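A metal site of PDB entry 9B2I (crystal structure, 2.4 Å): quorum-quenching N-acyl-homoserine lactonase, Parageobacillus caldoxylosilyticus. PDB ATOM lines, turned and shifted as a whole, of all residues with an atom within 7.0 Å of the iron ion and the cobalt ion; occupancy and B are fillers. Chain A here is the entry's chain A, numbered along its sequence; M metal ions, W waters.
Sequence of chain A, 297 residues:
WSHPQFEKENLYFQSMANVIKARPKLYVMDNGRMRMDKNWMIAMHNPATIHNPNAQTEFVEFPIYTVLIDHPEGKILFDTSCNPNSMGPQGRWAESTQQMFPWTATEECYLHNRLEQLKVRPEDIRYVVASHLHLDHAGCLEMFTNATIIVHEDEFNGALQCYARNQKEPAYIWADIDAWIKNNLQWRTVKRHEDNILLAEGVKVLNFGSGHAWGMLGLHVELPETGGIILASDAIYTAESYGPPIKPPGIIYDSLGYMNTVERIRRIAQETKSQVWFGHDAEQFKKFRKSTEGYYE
The side-chain carboxylate (OD2) of Asp 79 lies within hydrogen-bond range of a ring nitrogen (ND1) of His 137, 2.7 Å away. ND1 of His 280 is in hydrogen-bond range of O of Pro 63. A ring nitrogen (ND1) of His 132 lies within hydrogen-bond range of the side-chain hydroxyl (OG) of Ser 131 (2.8 Å). N of His 280 sits at hydrogen-bond distance from O of Tyr 237 (3.0 Å). ND1 of His 212 is in hydrogen-bond range of O of Ile 251.
Four residues have an atom within 4 Å of the iron ion: Asp 136, His 137, Asp 234 and His 280. The nearest printed residue that does not touch the iron ion is His 132 (4.4 Å).
The nearest printed residue that does not touch the cobalt ion is His 137 (4.2 Å).
The iron ion is bound by a ring nitrogen (NE2) of His 137 (2.0 Å), a ring nitrogen (NE2) of His 280 (2.1 Å), water W1 (2.1 Å), the side-chain carboxylate (OD2) of Asp 136 (2.3 Å), water W2 (2.3 Å) and the side-chain carboxylate (OD2) of Asp 234 (2.3 Å). The iron ion has six donor atoms within binding distance. Slightly farther from the iron ion lies OD1 of Asp 234 (2.7 Å).
The cobalt ion is bound by OD2 of Asp 234 (2.0 Å), ND1 of His 134 (2.0 Å), water W3 (2.1 Å), NE2 of His 212 (2.1 Å), NE2 of His 132 (2.2 Å) and water W2 (2.3 Å). The cobalt ion has six donor atoms within binding distance.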
ATOM      1  N   MET A  34     -13.103 -21.065  17.923  1.00  0.00           N
ATOM      2  CA  MET A  34     -14.417 -21.090  18.554  1.00  0.00           C
ATOM      3  C   MET A  34     -14.927 -19.659  18.671  1.00  0.00           C
ATOM      4  O   MET A  34     -14.139 -18.725  18.738  1.00  0.00           O
ATOM      5  CB  MET A  34     -14.347 -21.744  19.934  1.00  0.00           C
ATOM      6  CG  MET A  34     -15.698 -22.012  20.575  1.00  0.00           C
ATOM      7  SD  MET A  34     -15.557 -22.949  22.119  1.00  0.00           S
ATOM      8  CE  MET A  34     -15.203 -24.571  21.438  1.00  0.00           C
ATOM      9  N   PHE A  62     -11.889 -17.116  18.917  1.00  0.00           N
ATOM     10  CA  PHE A  62     -10.682 -17.362  19.677  1.00  0.00           C
ATOM     11  C   PHE A  62     -10.103 -18.721  19.311  1.00  0.00           C
ATOM     12  O   PHE A  62     -10.831 -19.623  18.903  1.00  0.00           O
ATOM     13  CB  PHE A  62     -10.947 -17.249  21.179  1.00  0.00           C
ATOM     14  CG  PHE A  62     -12.079 -18.117  21.719  1.00  0.00           C
ATOM     15  CD1 PHE A  62     -13.389 -17.643  21.752  1.00  0.00           C
ATOM     16  CD2 PHE A  62     -11.832 -19.396  22.212  1.00  0.00           C
ATOM     17  CE1 PHE A  62     -14.414 -18.428  22.262  1.00  0.00           C
ATOM     18  CE2 PHE A  62     -12.862 -20.172  22.707  1.00  0.00           C
ATOM     19  CZ  PHE A  62     -14.147 -19.688  22.730  1.00  0.00           C
ATOM     20  N   PRO A  63      -8.766 -18.907  19.440  1.00  0.00           N
ATOM     21  CA  PRO A  63      -8.129 -20.178  19.119  1.00  0.00           C
ATOM     22  C   PRO A  63      -8.235 -21.231  20.205  1.00  0.00           C
ATOM     23  O   PRO A  63      -8.052 -20.952  21.390  1.00  0.00           O
ATOM     24  CB  PRO A  63      -6.663 -19.757  18.881  1.00  0.00           C
ATOM     25  CG  PRO A  63      -6.466 -18.584  19.827  1.00  0.00           C
ATOM     26  CD  PRO A  63      -7.812 -17.870  19.860  1.00  0.00           C
ATOM     27  N   ILE A  64      -8.556 -22.454  19.782  1.00  0.00           N
ATOM     28  CA  ILE A  64      -8.372 -23.647  20.595  1.00  0.00           C
ATOM     29  C   ILE A  64      -7.019 -24.250  20.223  1.00  0.00           C
ATOM     30  O   ILE A  64      -6.744 -24.453  19.044  1.00  0.00           O
ATOM     31  CB  ILE A  64      -9.508 -24.658  20.340  1.00  0.00           C
ATOM     32  CG1 ILE A  64     -10.879 -23.988  20.365  1.00  0.00           C
ATOM     33  CG2 ILE A  64      -9.421 -25.842  21.306  1.00  0.00           C
ATOM     34  CD1 ILE A  64     -11.153 -23.183  21.628  1.00  0.00           C
ATOM     35  N   ASP A  79      -3.694 -30.349  27.518  1.00  0.00           N
ATOM     36  CA  ASP A  79      -5.005 -30.145  26.911  1.00  0.00           C
ATOM     37  C   ASP A  79      -5.141 -31.049  25.688  1.00  0.00           C
ATOM     38  O   ASP A  79      -4.169 -31.658  25.254  1.00  0.00           O
ATOM     39  CB  ASP A  79      -5.259 -28.667  26.625  1.00  0.00           C
ATOM     40  CG  ASP A  79      -5.706 -27.847  27.825  1.00  0.00           C
ATOM     41  OD1 ASP A  79      -5.958 -28.438  28.888  1.00  0.00           O
ATOM     42  OD2 ASP A  79      -5.792 -26.608  27.681  1.00  0.00           O
ATOM     43  N   SER A 131      -6.038 -29.273  31.800  1.00  0.00           N
ATOM     44  CA  SER A 131      -6.157 -28.026  32.530  1.00  0.00           C
ATOM     45  C   SER A 131      -7.480 -28.029  33.290  1.00  0.00           C
ATOM     46  O   SER A 131      -7.535 -27.673  34.466  1.00  0.00           O
ATOM     47  CB  SER A 131      -6.056 -26.837  31.612  1.00  0.00           C
ATOM     48  OG  SER A 131      -7.147 -26.800  30.699  1.00  0.00           O
ATOM     49  N   HIS A 132      -8.539 -28.434  32.588  1.00  0.00           N
ATOM     50  CA  HIS A 132      -9.857 -28.676  33.154  1.00  0.00           C
ATOM     51  C   HIS A 132     -10.618 -29.543  32.160  1.00  0.00           C
ATOM     52  O   HIS A 132     -10.035 -30.002  31.181  1.00  0.00           O
ATOM     53  CB  HIS A 132     -10.545 -27.353  33.525  1.00  0.00           C
ATOM     54  CG  HIS A 132     -10.700 -26.378  32.395  1.00  0.00           C
ATOM     55  ND1 HIS A 132      -9.683 -26.049  31.532  1.00  0.00           N
ATOM     56  CD2 HIS A 132     -11.757 -25.645  32.033  1.00  0.00           C
ATOM     57  CE1 HIS A 132     -10.120 -25.157  30.660  1.00  0.00           C
ATOM     58  NE2 HIS A 132     -11.384 -24.899  30.941  1.00  0.00           N
ATOM     59  N   LEU A 133     -11.905 -29.783  32.406  1.00  0.00           N
ATOM     60  CA  LEU A 133     -12.625 -30.778  31.629  1.00  0.00           C
ATOM     61  C   LEU A 133     -13.734 -30.132  30.791  1.00  0.00           C
ATOM     62  O   LEU A 133     -14.725 -30.780  30.461  1.00  0.00           O
ATOM     63  CB  LEU A 133     -13.175 -31.848  32.578  1.00  0.00           C
ATOM     64  CG  LEU A 133     -12.112 -32.680  33.294  1.00  0.00           C
ATOM     65  CD1 LEU A 133     -12.759 -33.696  34.225  1.00  0.00           C
ATOM     66  CD2 LEU A 133     -11.189 -33.373  32.307  1.00  0.00           C
ATOM     67  N   HIS A 134     -13.526 -28.867  30.421  1.00  0.00           N
ATOM     68  CA  HIS A 134     -14.409 -28.185  29.501  1.00  0.00           C
ATOM     69  C   HIS A 134     -14.306 -28.828  28.121  1.00  0.00           C
ATOM     70  O   HIS A 134     -13.324 -29.516  27.820  1.00  0.00           O
ATOM     71  CB  HIS A 134     -14.101 -26.684  29.454  1.00  0.00           C
ATOM     72  CG  HIS A 134     -14.727 -25.895  30.546  1.00  0.00           C
ATOM     73  ND1 HIS A 134     -14.418 -24.578  30.790  1.00  0.00           N
ATOM     74  CD2 HIS A 134     -15.682 -26.218  31.439  1.00  0.00           C
ATOM     75  CE1 HIS A 134     -15.152 -24.133  31.808  1.00  0.00           C
ATOM     76  NE2 HIS A 134     -15.921 -25.124  32.221  1.00  0.00           N
ATOM     77  N   LEU A 135     -15.310 -28.568  27.282  1.00  0.00           N
ATOM     78  CA  LEU A 135     -15.477 -29.237  26.006  1.00  0.00           C
ATOM     79  C   LEU A 135     -14.301 -28.955  25.079  1.00  0.00           C
ATOM     80  O   LEU A 135     -13.952 -29.787  24.245  1.00  0.00           O
ATOM     81  CB  LEU A 135     -16.800 -28.804  25.379  1.00  0.00           C
ATOM     82  CG  LEU A 135     -16.912 -27.340  24.962  1.00  0.00           C
ATOM     83  CD1 LEU A 135     -18.266 -27.081  24.319  1.00  0.00           C
ATOM     84  CD2 LEU A 135     -16.708 -26.388  26.126  1.00  0.00           C
ATOM     85  N   ASP A 136     -13.672 -27.779  25.243  1.00  0.00           N
ATOM     86  CA  ASP A 136     -12.650 -27.324  24.319  1.00  0.00           C
ATOM     87  C   ASP A 136     -11.256 -27.598  24.882  1.00  0.00           C
ATOM     88  O   ASP A 136     -10.273 -27.012  24.432  1.00  0.00           O
ATOM     89  CB  ASP A 136     -12.810 -25.854  24.001  1.00  0.00           C
ATOM     90  CG  ASP A 136     -12.814 -24.929  25.210  1.00  0.00           C
ATOM     91  OD1 ASP A 136     -13.567 -25.225  26.166  1.00  0.00           O
ATOM     92  OD2 ASP A 136     -12.071 -23.924  25.195  1.00  0.00           O
ATOM     93  N   HIS A 137     -11.174 -28.499  25.871  1.00  0.00           N
ATOM     94  CA  HIS A 137      -9.902 -28.825  26.490  1.00  0.00           C
ATOM     95  C   HIS A 137      -9.786 -30.324  26.743  1.00  0.00           C
ATOM     96  O   HIS A 137      -8.681 -30.877  26.738  1.00  0.00           O
ATOM     97  CB  HIS A 137      -9.713 -28.042  27.790  1.00  0.00           C
ATOM     98  CG  HIS A 137      -9.617 -26.565  27.609  1.00  0.00           C
ATOM     99  ND1 HIS A 137      -8.422 -25.894  27.512  1.00  0.00           N
ATOM    100  CD2 HIS A 137     -10.573 -25.631  27.506  1.00  0.00           C
ATOM    101  CE1 HIS A 137      -8.652 -24.594  27.350  1.00  0.00           C
ATOM    102  NE2 HIS A 137      -9.960 -24.415  27.347  1.00  0.00           N
ATOM    103  N   GLU A 155     -12.362 -31.037  39.640  1.00  0.00           N
ATOM    104  CA  GLU A 155     -12.855 -30.928  38.279  1.00  0.00           C
ATOM    105  C   GLU A 155     -13.398 -32.276  37.834  1.00  0.00           C
ATOM    106  O   GLU A 155     -14.452 -32.362  37.192  1.00  0.00           O
ATOM    107  CB  GLU A 155     -11.739 -30.459  37.344  1.00  0.00           C
ATOM    108  CG  GLU A 155     -12.214 -30.203  35.915  1.00  0.00           C
ATOM    109  CD  GLU A 155     -13.045 -28.947  35.741  1.00  0.00           C
ATOM    110  OE1 GLU A 155     -13.205 -28.192  36.729  1.00  0.00           O
ATOM    111  OE2 GLU A 155     -13.554 -28.726  34.621  1.00  0.00           O
ATOM    112  N   ALA A 171     -20.828 -26.790  29.170  1.00  0.00           N
ATOM    113  CA  ALA A 171     -19.376 -26.835  29.010  1.00  0.00           C
ATOM    114  C   ALA A 171     -18.845 -28.259  29.172  1.00  0.00           C
ATOM    115  O   ALA A 171     -17.711 -28.530  28.817  1.00  0.00           O
ATOM    116  CB  ALA A 171     -18.727 -25.885  29.990  1.00  0.00           C
ATOM    117  N   TYR A 172     -19.689 -29.152  29.698  1.00  0.00           N
ATOM    118  CA  TYR A 172     -19.262 -30.524  29.950  1.00  0.00           C
ATOM    119  C   TYR A 172     -20.085 -31.464  29.075  1.00  0.00           C
ATOM    120  O   TYR A 172     -21.314 -31.484  29.157  1.00  0.00           O
ATOM    121  CB  TYR A 172     -19.362 -30.825  31.448  1.00  0.00           C
ATOM    122  CG  TYR A 172     -18.422 -29.980  32.308  1.00  0.00           C
ATOM    123  CD1 TYR A 172     -17.124 -30.388  32.565  1.00  0.00           C
ATOM    124  CD2 TYR A 172     -18.841 -28.776  32.862  1.00  0.00           C
ATOM    125  CE1 TYR A 172     -16.266 -29.627  33.335  1.00  0.00           C
ATOM    126  CE2 TYR A 172     -17.997 -28.005  33.635  1.00  0.00           C
ATOM    127  CZ  TYR A 172     -16.703 -28.424  33.881  1.00  0.00           C
ATOM    128  OH  TYR A 172     -15.863 -27.675  34.643  1.00  0.00           O
ATOM    129  N   HIS A 212     -11.988 -20.414  37.366  1.00  0.00           N
ATOM    130  CA  HIS A 212     -12.723 -20.518  36.112  1.00  0.00           C
ATOM    131  C   HIS A 212     -13.642 -21.729  36.188  1.00  0.00           C
ATOM    132  O   HIS A 212     -14.816 -21.645  35.833  1.00  0.00           O
ATOM    133  CB  HIS A 212     -11.747 -20.592  34.932  1.00  0.00           C
ATOM    134  CG  HIS A 212     -12.358 -21.015  33.648  1.00  0.00           C
ATOM    135  ND1 HIS A 212     -13.123 -20.173  32.865  1.00  0.00           N
ATOM    136  CD2 HIS A 212     -12.331 -22.189  33.001  1.00  0.00           C
ATOM    137  CE1 HIS A 212     -13.530 -20.828  31.784  1.00  0.00           C
ATOM    138  NE2 HIS A 212     -13.060 -22.053  31.847  1.00  0.00           N
ATOM    139  N   ALA A 213     -13.082 -22.853  36.645  1.00  0.00           N
ATOM    140  CA  ALA A 213     -13.837 -24.085  36.825  1.00  0.00           C
ATOM    141  C   ALA A 213     -13.556 -24.667  38.214  1.00  0.00           C
ATOM    142  O   ALA A 213     -12.915 -24.023  39.041  1.00  0.00           O
ATOM    143  CB  ALA A 213     -13.492 -25.071  35.730  1.00  0.00           C
ATOM    144  N   MET A 216      -8.505 -26.187  38.332  1.00  0.00           N
ATOM    145  CA  MET A 216      -7.669 -25.801  37.210  1.00  0.00           C
ATOM    146  C   MET A 216      -6.235 -26.253  37.448  1.00  0.00           C
ATOM    147  O   MET A 216      -5.710 -26.113  38.552  1.00  0.00           O
ATOM    148  CB  MET A 216      -7.687 -24.280  37.026  1.00  0.00           C
ATOM    149  CG  MET A 216      -9.078 -23.685  36.900  1.00  0.00           C
ATOM    150  SD  MET A 216      -9.897 -24.132  35.360  1.00  0.00           S
ATOM    151  CE  MET A 216      -8.787 -23.375  34.169  1.00  0.00           C
ATOM    152  N   SER A 233      -3.847 -21.735  30.531  1.00  0.00           N
ATOM    153  CA  SER A 233      -5.138 -22.203  30.044  1.00  0.00           C
ATOM    154  C   SER A 233      -6.213 -21.184  30.402  1.00  0.00           C
ATOM    155  O   SER A 233      -5.978 -19.980  30.338  1.00  0.00           O
ATOM    156  CB  SER A 233      -5.450 -23.579  30.583  1.00  0.00           C
ATOM    157  OG  SER A 233      -6.708 -24.044  30.100  1.00  0.00           O
ATOM    158  N   ASP A 234      -7.380 -21.672  30.823  1.00  0.00           N
ATOM    159  CA  ASP A 234      -8.543 -20.823  31.026  1.00  0.00           C
ATOM    160  C   ASP A 234      -8.471 -20.112  32.375  1.00  0.00           C
ATOM    161  O   ASP A 234      -9.403 -19.415  32.756  1.00  0.00           O
ATOM    162  CB  ASP A 234      -9.843 -21.590  30.899  1.00  0.00           C
ATOM    163  CG  ASP A 234     -10.262 -21.944  29.481  1.00  0.00           C
ATOM    164  OD1 ASP A 234      -9.510 -21.616  28.545  1.00  0.00           O
ATOM    165  OD2 ASP A 234     -11.352 -22.541  29.323  1.00  0.00           O
ATOM    166  N   ALA A 235      -7.371 -20.286  33.111  1.00  0.00           N
ATOM    167  CA  ALA A 235      -7.118 -19.490  34.298  1.00  0.00           C
ATOM    168  C   ALA A 235      -7.015 -18.024  33.874  1.00  0.00           C
ATOM    169  O   ALA A 235      -7.374 -17.121  34.621  1.00  0.00           O
ATOM    170  CB  ALA A 235      -5.876 -19.959  35.011  1.00  0.00           C
ATOM    171  N   TYR A 237      -7.948 -16.130  30.189  1.00  0.00           N
ATOM    172  CA  TYR A 237      -8.439 -16.231  28.820  1.00  0.00           C
ATOM    173  C   TYR A 237      -7.522 -15.473  27.869  1.00  0.00           C
ATOM    174  O   TYR A 237      -7.059 -16.031  26.883  1.00  0.00           O
ATOM    175  CB  TYR A 237      -9.867 -15.675  28.734  1.00  0.00           C
ATOM    176  CG  TYR A 237     -11.025 -16.655  28.935  1.00  0.00           C
ATOM    177  CD1 TYR A 237     -10.894 -18.011  28.663  1.00  0.00           C
ATOM    178  CD2 TYR A 237     -12.266 -16.202  29.360  1.00  0.00           C
ATOM    179  CE1 TYR A 237     -11.955 -18.889  28.827  1.00  0.00           C
ATOM    180  CE2 TYR A 237     -13.332 -17.060  29.531  1.00  0.00           C
ATOM    181  CZ  TYR A 237     -13.174 -18.413  29.272  1.00  0.00           C
ATOM    182  OH  TYR A 237     -14.228 -19.260  29.437  1.00  0.00           O
ATOM    183  N   ILE A 251     -17.975 -16.944  32.398  1.00  0.00           N
ATOM    184  CA  ILE A 251     -17.809 -18.352  32.737  1.00  0.00           C
ATOM    185  C   ILE A 251     -16.873 -18.432  33.934  1.00  0.00           C
ATOM    186  O   ILE A 251     -15.679 -18.177  33.808  1.00  0.00           O
ATOM    187  CB  ILE A 251     -17.259 -19.174  31.554  1.00  0.00           C
ATOM    188  CG1 ILE A 251     -18.153 -19.066  30.309  1.00  0.00           C
ATOM    189  CG2 ILE A 251     -17.054 -20.624  31.959  1.00  0.00           C
ATOM    190  CD1 ILE A 251     -17.824 -20.081  29.231  1.00  0.00           C
ATOM    191  N   GLY A 279      -5.002 -18.985  27.429  1.00  0.00           N
ATOM    192  CA  GLY A 279      -5.709 -20.139  26.892  1.00  0.00           C
ATOM    193  C   GLY A 279      -6.346 -19.845  25.537  1.00  0.00           C
ATOM    194  O   GLY A 279      -6.432 -20.742  24.696  1.00  0.00           O
ATOM    195  N   HIS A 280      -6.770 -18.601  25.329  1.00  0.00           N
ATOM    196  CA  HIS A 280      -7.576 -18.269  24.157  1.00  0.00           C
ATOM    197  C   HIS A 280      -7.343 -16.818  23.720  1.00  0.00           C
ATOM    198  O   HIS A 280      -8.295 -16.087  23.488  1.00  0.00           O
ATOM    199  CB  HIS A 280      -9.066 -18.464  24.469  1.00  0.00           C
ATOM    200  CG  HIS A 280      -9.433 -19.855  24.870  1.00  0.00           C
ATOM    201  ND1 HIS A 280      -9.138 -20.974  24.116  1.00  0.00           N
ATOM    202  CD2 HIS A 280     -10.105 -20.298  25.941  1.00  0.00           C
ATOM    203  CE1 HIS A 280      -9.608 -22.050  24.737  1.00  0.00           C
ATOM    204  NE2 HIS A 280     -10.203 -21.659  25.848  1.00  0.00           N
HETATM  205 FE    FE M   1     -11.308 -22.927  27.063  1.00  0.00          FE
HETATM  206 CO    CO M   2     -12.830 -23.444  30.243  1.00  0.00          CO
HETATM  207  O   HOH W   1     -12.834 -21.434  27.148  1.00  0.00           O
HETATM  208  O   HOH W   2     -13.176 -23.807  28.025  1.00  0.00           O
HETATM  209  O   HOH W   3     -13.883 -21.973  29.256  1.00  0.00           O
